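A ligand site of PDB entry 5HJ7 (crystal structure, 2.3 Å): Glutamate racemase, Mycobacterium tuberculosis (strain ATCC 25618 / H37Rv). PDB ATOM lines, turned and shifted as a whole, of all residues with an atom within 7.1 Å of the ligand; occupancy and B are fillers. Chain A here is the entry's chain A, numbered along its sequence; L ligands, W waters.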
ATOM      1  N   ASP A  14      10.178  -3.502  23.410  1.00  0.00           N
ATOM      2  CA  ASP A  14       9.627  -4.790  23.797  1.00  0.00           C
ATOM      3  C   ASP A  14       8.124  -4.668  23.791  1.00  0.00           C
ATOM      4  O   ASP A  14       7.563  -3.577  23.756  1.00  0.00           O
ATOM      5  CB  ASP A  14      10.145  -5.197  25.186  1.00  0.00           C
ATOM      6  CG  ASP A  14       9.595  -6.544  25.637  1.00  0.00           C
ATOM      7  OD1 ASP A  14       9.829  -7.548  24.942  1.00  0.00           O
ATOM      8  OD2 ASP A  14       8.895  -6.594  26.684  1.00  0.00           O
ATOM      9  N   SER A  15       7.464  -5.829  23.825  1.00  0.00           N
ATOM     10  CA  SER A  15       6.026  -5.884  23.981  1.00  0.00           C
ATOM     11  C   SER A  15       5.550  -5.301  25.302  1.00  0.00           C
ATOM     12  O   SER A  15       4.384  -4.917  25.422  1.00  0.00           O
ATOM     13  CB  SER A  15       5.572  -7.334  23.894  1.00  0.00           C
ATOM     14  OG  SER A  15       5.995  -8.039  25.057  1.00  0.00           O
ATOM     15  N   GLY A  16       6.417  -5.253  26.319  1.00  0.00           N
ATOM     16  CA  GLY A  16       5.980  -4.840  27.640  1.00  0.00           C
ATOM     17  C   GLY A  16       7.133  -4.645  28.607  1.00  0.00           C
ATOM     18  O   GLY A  16       8.060  -3.885  28.336  1.00  0.00           O
ATOM     19  N   VAL A  17       7.077  -5.364  29.730  1.00  0.00           N
ATOM     20  CA  VAL A  17       8.081  -5.214  30.785  1.00  0.00           C
ATOM     21  C   VAL A  17       9.146  -6.305  30.724  1.00  0.00           C
ATOM     22  O   VAL A  17      10.259  -6.105  31.241  1.00  0.00           O
ATOM     23  CB  VAL A  17       7.404  -5.204  32.174  1.00  0.00           C
ATOM     24  CG1 VAL A  17       8.385  -4.799  33.249  1.00  0.00           C
ATOM     25  CG2 VAL A  17       6.252  -4.244  32.181  1.00  0.00           C
ATOM     26  N   GLY A  18       8.847  -7.459  30.111  1.00  0.00           N
ATOM     27  CA  GLY A  18       9.787  -8.571  30.115  1.00  0.00           C
ATOM     28  C   GLY A  18      11.059  -8.296  29.343  1.00  0.00           C
ATOM     29  O   GLY A  18      12.098  -8.902  29.607  1.00  0.00           O
ATOM     30  N   GLY A  19      11.002  -7.380  28.374  1.00  0.00           N
ATOM     31  CA  GLY A  19      12.214  -7.013  27.659  1.00  0.00           C
ATOM     32  C   GLY A  19      13.259  -6.361  28.530  1.00  0.00           C
ATOM     33  O   GLY A  19      14.394  -6.174  28.080  1.00  0.00           O
ATOM     34  N   GLY A  44       0.365  -4.690  24.203  1.00  0.00           N
ATOM     35  CA  GLY A  44       0.685  -6.096  24.364  1.00  0.00           C
ATOM     36  C   GLY A  44      -0.245  -6.786  25.341  1.00  0.00           C
ATOM     37  O   GLY A  44      -1.191  -6.161  25.808  1.00  0.00           O
ATOM     38  N   PRO A  45       0.000  -8.072  25.667  1.00  0.00           N
ATOM     39  CA  PRO A  45       1.093  -8.943  25.191  1.00  0.00           C
ATOM     40  C   PRO A  45       1.045  -9.235  23.703  1.00  0.00           C
ATOM     41  O   PRO A  45      -0.038  -9.249  23.130  1.00  0.00           O
ATOM     42  CB  PRO A  45       0.883 -10.246  25.967  1.00  0.00           C
ATOM     43  CG  PRO A  45      -0.583 -10.224  26.376  1.00  0.00           C
ATOM     44  CD  PRO A  45      -0.858  -8.765  26.642  1.00  0.00           C
ATOM     45  N   TYR A  46       2.215  -9.461  23.090  1.00  0.00           N
ATOM     46  CA  TYR A  46       2.273  -9.833  21.678  1.00  0.00           C
ATOM     47  C   TYR A  46       2.065 -11.322  21.478  1.00  0.00           C
ATOM     48  O   TYR A  46       1.645 -11.743  20.386  1.00  0.00           O
ATOM     49  CB  TYR A  46       3.622  -9.447  21.071  1.00  0.00           C
ATOM     50  CG  TYR A  46       3.877  -7.972  20.909  1.00  0.00           C
ATOM     51  CD1 TYR A  46       2.875  -7.039  21.076  1.00  0.00           C
ATOM     52  CD2 TYR A  46       5.151  -7.520  20.567  1.00  0.00           C
ATOM     53  CE1 TYR A  46       3.127  -5.687  20.902  1.00  0.00           C
ATOM     54  CE2 TYR A  46       5.420  -6.177  20.400  1.00  0.00           C
ATOM     55  CZ  TYR A  46       4.411  -5.264  20.557  1.00  0.00           C
ATOM     56  OH  TYR A  46       4.710  -3.929  20.395  1.00  0.00           O
ATOM     57  N   GLY A  47       2.364 -12.134  22.503  1.00  0.00           N
ATOM     58  CA  GLY A  47       2.212 -13.573  22.469  1.00  0.00           C
ATOM     59  C   GLY A  47       1.009 -14.130  21.722  1.00  0.00           C
ATOM     60  O   GLY A  47       1.148 -15.013  20.863  1.00  0.00           O
ATOM     61  N   PRO A  48      -0.200 -13.664  22.051  1.00  0.00           N
ATOM     62  CA  PRO A  48      -1.413 -14.190  21.399  1.00  0.00           C
ATOM     63  C   PRO A  48      -1.868 -13.432  20.152  1.00  0.00           C
ATOM     64  O   PRO A  48      -2.921 -13.767  19.603  1.00  0.00           O
ATOM     65  CB  PRO A  48      -2.458 -14.083  22.515  1.00  0.00           C
ATOM     66  CG  PRO A  48      -2.070 -12.829  23.223  1.00  0.00           C
ATOM     67  CD  PRO A  48      -0.553 -12.794  23.198  1.00  0.00           C
ATOM     68  N   ALA A  76      14.057  -6.336  21.545  1.00  0.00           N
ATOM     69  CA  ALA A  76      14.258  -7.215  22.685  1.00  0.00           C
ATOM     70  C   ALA A  76      13.199  -8.292  22.762  1.00  0.00           C
ATOM     71  O   ALA A  76      13.427  -9.346  23.378  1.00  0.00           O
ATOM     72  CB  ALA A  76      14.295  -6.375  23.967  1.00  0.00           C
ATOM     73  N   CYS A  77      12.057  -8.081  22.105  1.00  0.00           N
ATOM     74  CA  CYS A  77      10.952  -9.030  22.113  1.00  0.00           C
ATOM     75  C   CYS A  77      11.153 -10.109  21.049  1.00  0.00           C
ATOM     76  O   CYS A  77      11.441  -9.791  19.888  1.00  0.00           O
ATOM     77  CB  CYS A  77       9.648  -8.273  21.867  1.00  0.00           C
ATOM     78  SG  CYS A  77       8.171  -9.268  21.857  1.00  0.00           S
ATOM     79  N   ASN A  78      11.017 -11.377  21.434  1.00  0.00           N
ATOM     80  CA  ASN A  78      11.148 -12.441  20.441  1.00  0.00           C
ATOM     81  C   ASN A  78       9.944 -12.499  19.517  1.00  0.00           C
ATOM     82  O   ASN A  78      10.090 -12.882  18.346  1.00  0.00           O
ATOM     83  CB  ASN A  78      11.316 -13.801  21.112  1.00  0.00           C
ATOM     84  CG  ASN A  78      12.524 -13.871  21.974  1.00  0.00           C
ATOM     85  OD1 ASN A  78      12.523 -13.318  23.083  1.00  0.00           O
ATOM     86  ND2 ASN A  78      13.577 -14.520  21.482  1.00  0.00           N
ATOM     87  N   SER A  79       8.759 -12.145  20.019  1.00  0.00           N
ATOM     88  CA  SER A  79       7.589 -12.094  19.158  1.00  0.00           C
ATOM     89  C   SER A  79       7.691 -10.956  18.161  1.00  0.00           C
ATOM     90  O   SER A  79       7.324 -11.121  16.990  1.00  0.00           O
ATOM     91  CB  SER A  79       6.301 -11.941  19.985  1.00  0.00           C
ATOM     92  OG  SER A  79       6.178 -12.984  20.955  1.00  0.00           O
ATOM     93  N   ALA A  80       8.156  -9.791  18.597  1.00  0.00           N
ATOM     94  CA  ALA A  80       8.305  -8.678  17.658  1.00  0.00           C
ATOM     95  C   ALA A  80       9.422  -8.965  16.653  1.00  0.00           C
ATOM     96  O   ALA A  80       9.315  -8.597  15.484  1.00  0.00           O
ATOM     97  CB  ALA A  80       8.566  -7.376  18.412  1.00  0.00           C
ATOM     98  N   VAL A  99      16.708 -10.619  18.885  1.00  0.00           N
ATOM     99  CA  VAL A  99      16.955 -11.657  19.881  1.00  0.00           C
ATOM    100  C   VAL A  99      16.887 -13.076  19.324  1.00  0.00           C
ATOM    101  O   VAL A  99      17.213 -14.021  20.052  1.00  0.00           O
ATOM    102  CB  VAL A  99      15.991 -11.509  21.090  1.00  0.00           C
ATOM    103  CG1 VAL A  99      16.420 -10.341  21.962  1.00  0.00           C
ATOM    104  CG2 VAL A  99      14.580 -11.298  20.607  1.00  0.00           C
ATOM    105  N   GLY A 120       8.862 -20.703  23.056  1.00  0.00           N
ATOM    106  CA  GLY A 120       8.480 -19.321  22.893  1.00  0.00           C
ATOM    107  C   GLY A 120       6.977 -19.176  22.947  1.00  0.00           C
ATOM    108  O   GLY A 120       6.243 -20.139  23.157  1.00  0.00           O
ATOM    109  N   THR A 121       6.511 -17.936  22.739  1.00  0.00           N
ATOM    110  CA  THR A 121       5.078 -17.700  22.658  1.00  0.00           C
ATOM    111  C   THR A 121       4.490 -18.415  21.432  1.00  0.00           C
ATOM    112  O   THR A 121       5.204 -18.882  20.538  1.00  0.00           O
ATOM    113  CB  THR A 121       4.776 -16.203  22.576  1.00  0.00           C
ATOM    114  OG1 THR A 121       5.358 -15.666  21.381  1.00  0.00           O
ATOM    115  CG2 THR A 121       5.344 -15.445  23.793  1.00  0.00           C
ATOM    116  N   THR A 124       5.542 -16.429  18.317  1.00  0.00           N
ATOM    117  CA  THR A 124       6.928 -16.692  17.923  1.00  0.00           C
ATOM    118  C   THR A 124       7.054 -18.062  17.258  1.00  0.00           C
ATOM    119  O   THR A 124       7.639 -18.181  16.178  1.00  0.00           O
ATOM    120  CB  THR A 124       7.853 -16.592  19.130  1.00  0.00           C
ATOM    121  OG1 THR A 124       7.956 -15.218  19.513  1.00  0.00           O
ATOM    122  CG2 THR A 124       9.253 -17.111  18.796  1.00  0.00           C
ATOM    123  N   VAL A 151       4.733 -17.060  30.404  1.00  0.00           N
ATOM    124  CA  VAL A 151       4.769 -15.611  30.582  1.00  0.00           C
ATOM    125  C   VAL A 151       3.940 -15.179  31.790  1.00  0.00           C
ATOM    126  O   VAL A 151       4.363 -14.321  32.586  1.00  0.00           O
ATOM    127  CB  VAL A 151       4.319 -14.903  29.287  1.00  0.00           C
ATOM    128  CG1 VAL A 151       3.738 -13.513  29.577  1.00  0.00           C
ATOM    129  CG2 VAL A 151       5.490 -14.785  28.312  1.00  0.00           C
ATOM    130  N   GLU A 155       5.446 -13.482  35.379  1.00  0.00           N
ATOM    131  CA  GLU A 155       5.024 -12.168  35.858  1.00  0.00           C
ATOM    132  C   GLU A 155       4.362 -12.257  37.226  1.00  0.00           C
ATOM    133  O   GLU A 155       4.559 -11.369  38.076  1.00  0.00           O
ATOM    134  CB  GLU A 155       4.081 -11.496  34.845  1.00  0.00           C
ATOM    135  CG  GLU A 155       4.704 -11.344  33.451  1.00  0.00           C
ATOM    136  CD  GLU A 155       3.945 -10.379  32.533  1.00  0.00           C
ATOM    137  OE1 GLU A 155       4.603  -9.692  31.706  1.00  0.00           O
ATOM    138  OE2 GLU A 155       2.704 -10.308  32.649  1.00  0.00           O
ATOM    139  N   GLY A 186      13.405 -18.773  23.855  1.00  0.00           N
ATOM    140  CA  GLY A 186      13.046 -17.804  22.831  1.00  0.00           C
ATOM    141  C   GLY A 186      11.947 -16.846  23.232  1.00  0.00           C
ATOM    142  O   GLY A 186      10.968 -16.669  22.489  1.00  0.00           O
ATOM    143  N   CYS A 187      12.097 -16.218  24.400  1.00  0.00           N
ATOM    144  CA  CYS A 187      11.095 -15.335  24.965  1.00  0.00           C
ATOM    145  C   CYS A 187      11.758 -14.479  26.026  1.00  0.00           C
ATOM    146  O   CYS A 187      12.638 -14.955  26.754  1.00  0.00           O
ATOM    147  CB  CYS A 187       9.925 -16.138  25.552  1.00  0.00           C
ATOM    148  SG  CYS A 187       8.573 -15.149  26.217  1.00  0.00           S
ATOM    149  N   THR A 188      11.313 -13.211  26.123  1.00  0.00           N
ATOM    150  CA  THR A 188      11.904 -12.273  27.091  1.00  0.00           C
ATOM    151  C   THR A 188      11.791 -12.775  28.519  1.00  0.00           C
ATOM    152  O   THR A 188      12.625 -12.419  29.353  1.00  0.00           O
ATOM    153  CB  THR A 188      11.200 -10.922  27.013  1.00  0.00           C
ATOM    154  OG1 THR A 188       9.783 -11.141  26.992  1.00  0.00           O
ATOM    155  CG2 THR A 188      11.628 -10.108  25.799  1.00  0.00           C
ATOM    156  N   HIS A 189      10.739 -13.542  28.816  1.00  0.00           N
ATOM    157  CA  HIS A 189      10.447 -13.917  30.199  1.00  0.00           C
ATOM    158  C   HIS A 189      11.197 -15.147  30.673  1.00  0.00           C
ATOM    159  O   HIS A 189      11.381 -15.305  31.880  1.00  0.00           O
ATOM    160  CB  HIS A 189       8.951 -14.180  30.392  1.00  0.00           C
ATOM    161  CG  HIS A 189       8.107 -12.949  30.346  1.00  0.00           C
ATOM    162  ND1 HIS A 189       8.223 -12.002  29.353  1.00  0.00           N
ATOM    163  CD2 HIS A 189       7.112 -12.516  31.166  1.00  0.00           C
ATOM    164  CE1 HIS A 189       7.345 -11.034  29.561  1.00  0.00           C
ATOM    165  NE2 HIS A 189       6.654 -11.318  30.651  1.00  0.00           N
ATOM    166  N   TYR A 190      11.649 -16.022  29.748  1.00  0.00           N
ATOM    167  CA  TYR A 190      12.102 -17.363  30.084  1.00  0.00           C
ATOM    168  C   TYR A 190      13.447 -17.479  30.819  1.00  0.00           C
ATOM    169  O   TYR A 190      13.698 -18.539  31.399  1.00  0.00           O
ATOM    170  CB  TYR A 190      12.190 -18.210  28.814  1.00  0.00           C
ATOM    171  CG  TYR A 190      10.862 -18.474  28.114  1.00  0.00           C
ATOM    172  CD1 TYR A 190       9.672 -17.907  28.592  1.00  0.00           C
ATOM    173  CD2 TYR A 190      10.798 -19.304  26.996  1.00  0.00           C
ATOM    174  CE1 TYR A 190       8.458 -18.140  27.951  1.00  0.00           C
ATOM    175  CE2 TYR A 190       9.592 -19.549  26.351  1.00  0.00           C
ATOM    176  CZ  TYR A 190       8.436 -18.959  26.835  1.00  0.00           C
ATOM    177  OH  TYR A 190       7.236 -19.185  26.200  1.00  0.00           O
HETATM  178  N1  LIG L   1       8.161 -10.110  25.023  1.00  0.00           N
HETATM  179  C1  LIG L   1       7.434 -11.286  24.558  1.00  0.00           C
HETATM  180  C2  LIG L   1       8.373 -12.228  23.863  1.00  0.00           C
HETATM  181  O1  LIG L   1       7.915 -13.085  23.067  1.00  0.00           O
HETATM  182  C3  LIG L   1       6.760 -12.005  25.730  1.00  0.00           C
HETATM  183  C4  LIG L   1       5.545 -11.281  26.299  1.00  0.00           C
HETATM  184  C5  LIG L   1       4.421 -11.119  25.301  1.00  0.00           C
HETATM  185  O2  LIG L   1       3.816 -12.141  24.894  1.00  0.00           O
HETATM  186  O3  LIG L   1       4.140  -9.959  24.926  1.00  0.00           O
HETATM  187  O4  LIG L   1       9.584 -12.140  24.087  1.00  0.00           O
HETATM  188  O   HOH W   1       8.426 -15.628  22.255  1.00  0.00           O
HETATM  189  O   HOH W   2       2.386 -14.171  26.128  1.00  0.00           O
HETATM  190  O   HOH W   3       4.380  -8.323  27.849  1.00  0.00           O
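The side-chain hydroxyl (OG) of Ser 15 is in hydrogen-bond range of an oxygen (O3) of the ligand, 2.7 Å away.
O3 of the ligand sits at hydrogen-bond distance from N of Tyr 46 (2.7 Å).
The backbone NH of Ser 79 lies within hydrogen-bond range of an oxygen (O1) of the ligand, 3.3 Å away.
O1 of the ligand lies within hydrogen-bond range of OG of Ser 79 (2.7 Å).
N of Thr 188 is in hydrogen-bond range of O4 of the ligand (2.9 Å).
The side-chain hydroxyl of Thr 188 sits at hydrogen-bond distance from a nitrogen (N1) of the ligand.
An oxygen (O2) of the ligand sits at hydrogen-bond distance from the backbone NH (N) of Gly 47 (2.8 Å).
The side-chain carboxylate of Asp 14 lies within salt-bridge range of a nitrogen (N1) of the ligand.
The backbone NH (N) of Asn 78 lies within hydrogen-bond range of an oxygen (O4) of the ligand.
The side-chain amide oxygen (OD1) of Asn 78 sits close to an oxygen (O4) of the ligand (3.3 Å).
The side-chain sulfur (SG) of Cys 77 sits at hydrogen-bond distance from a nitrogen (N1) of the ligand.
N of Ser 79 lies close to SG of Cys 77.
The side-chain hydroxyl (OG1) of Thr 124 lies close to the side-chain hydroxyl (OG) of Ser 79, at 3.2 Å.
The backbone NH (N) of Thr 188 is in hydrogen-bond range of the side-chain amide oxygen (OD1) of Asn 78 (3.3 Å).
OG1 of Thr 188 is in hydrogen-bond range of ND1 of His 189, at 3.0 Å.
N of Gly 19 sits at hydrogen-bond distance from OD2 of Asp 14, 2.8 Å away.
OD2 of Asp 14 lies within hydrogen-bond range of N of Gly 16 (2.8 Å).
The backbone NH (N) of Cys 187 lies close to the side-chain amide oxygen (OD1) of Asn 78 (3.2 Å).
OG1 of Thr 121 sits at hydrogen-bond distance from N of Thr 124, at 3.2 Å.
Pro 45 touches the ligand.
Thr 121 touches the ligand.
Cys 187 touches the ligand (CA to O4, 3.6 Å).
His 189 touches the ligand (CE1 to C4, 3.7 Å).
Hydrophobic or aromatic side chains within 4 Å of the ligand: Pro 45, Tyr 46 and His 189.
Within 4 Å of the ligand: Asp 14, Ser 15, Pro 45, Tyr 46, Gly 47, Cys 77, Asn 78, Ser 79, Thr 121, Cys 187, Thr 188 and His 189.
The nearest printed residue that does not touch the ligand is Val 151 (4.001 Å).
Water W1 lies within hydrogen-bond range of an oxygen (O1) of the ligand (2.7 Å), the backbone carbonyl oxygen of Gly 186 (2.8 Å), the side-chain hydroxyl of Thr 124 (2.8 Å) and the backbone NH of Thr 121 (3.0 Å).
Water W3 bridges the side-chain hydroxyl (OG) of Ser 15 and an oxygen (O3) of the ligand.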
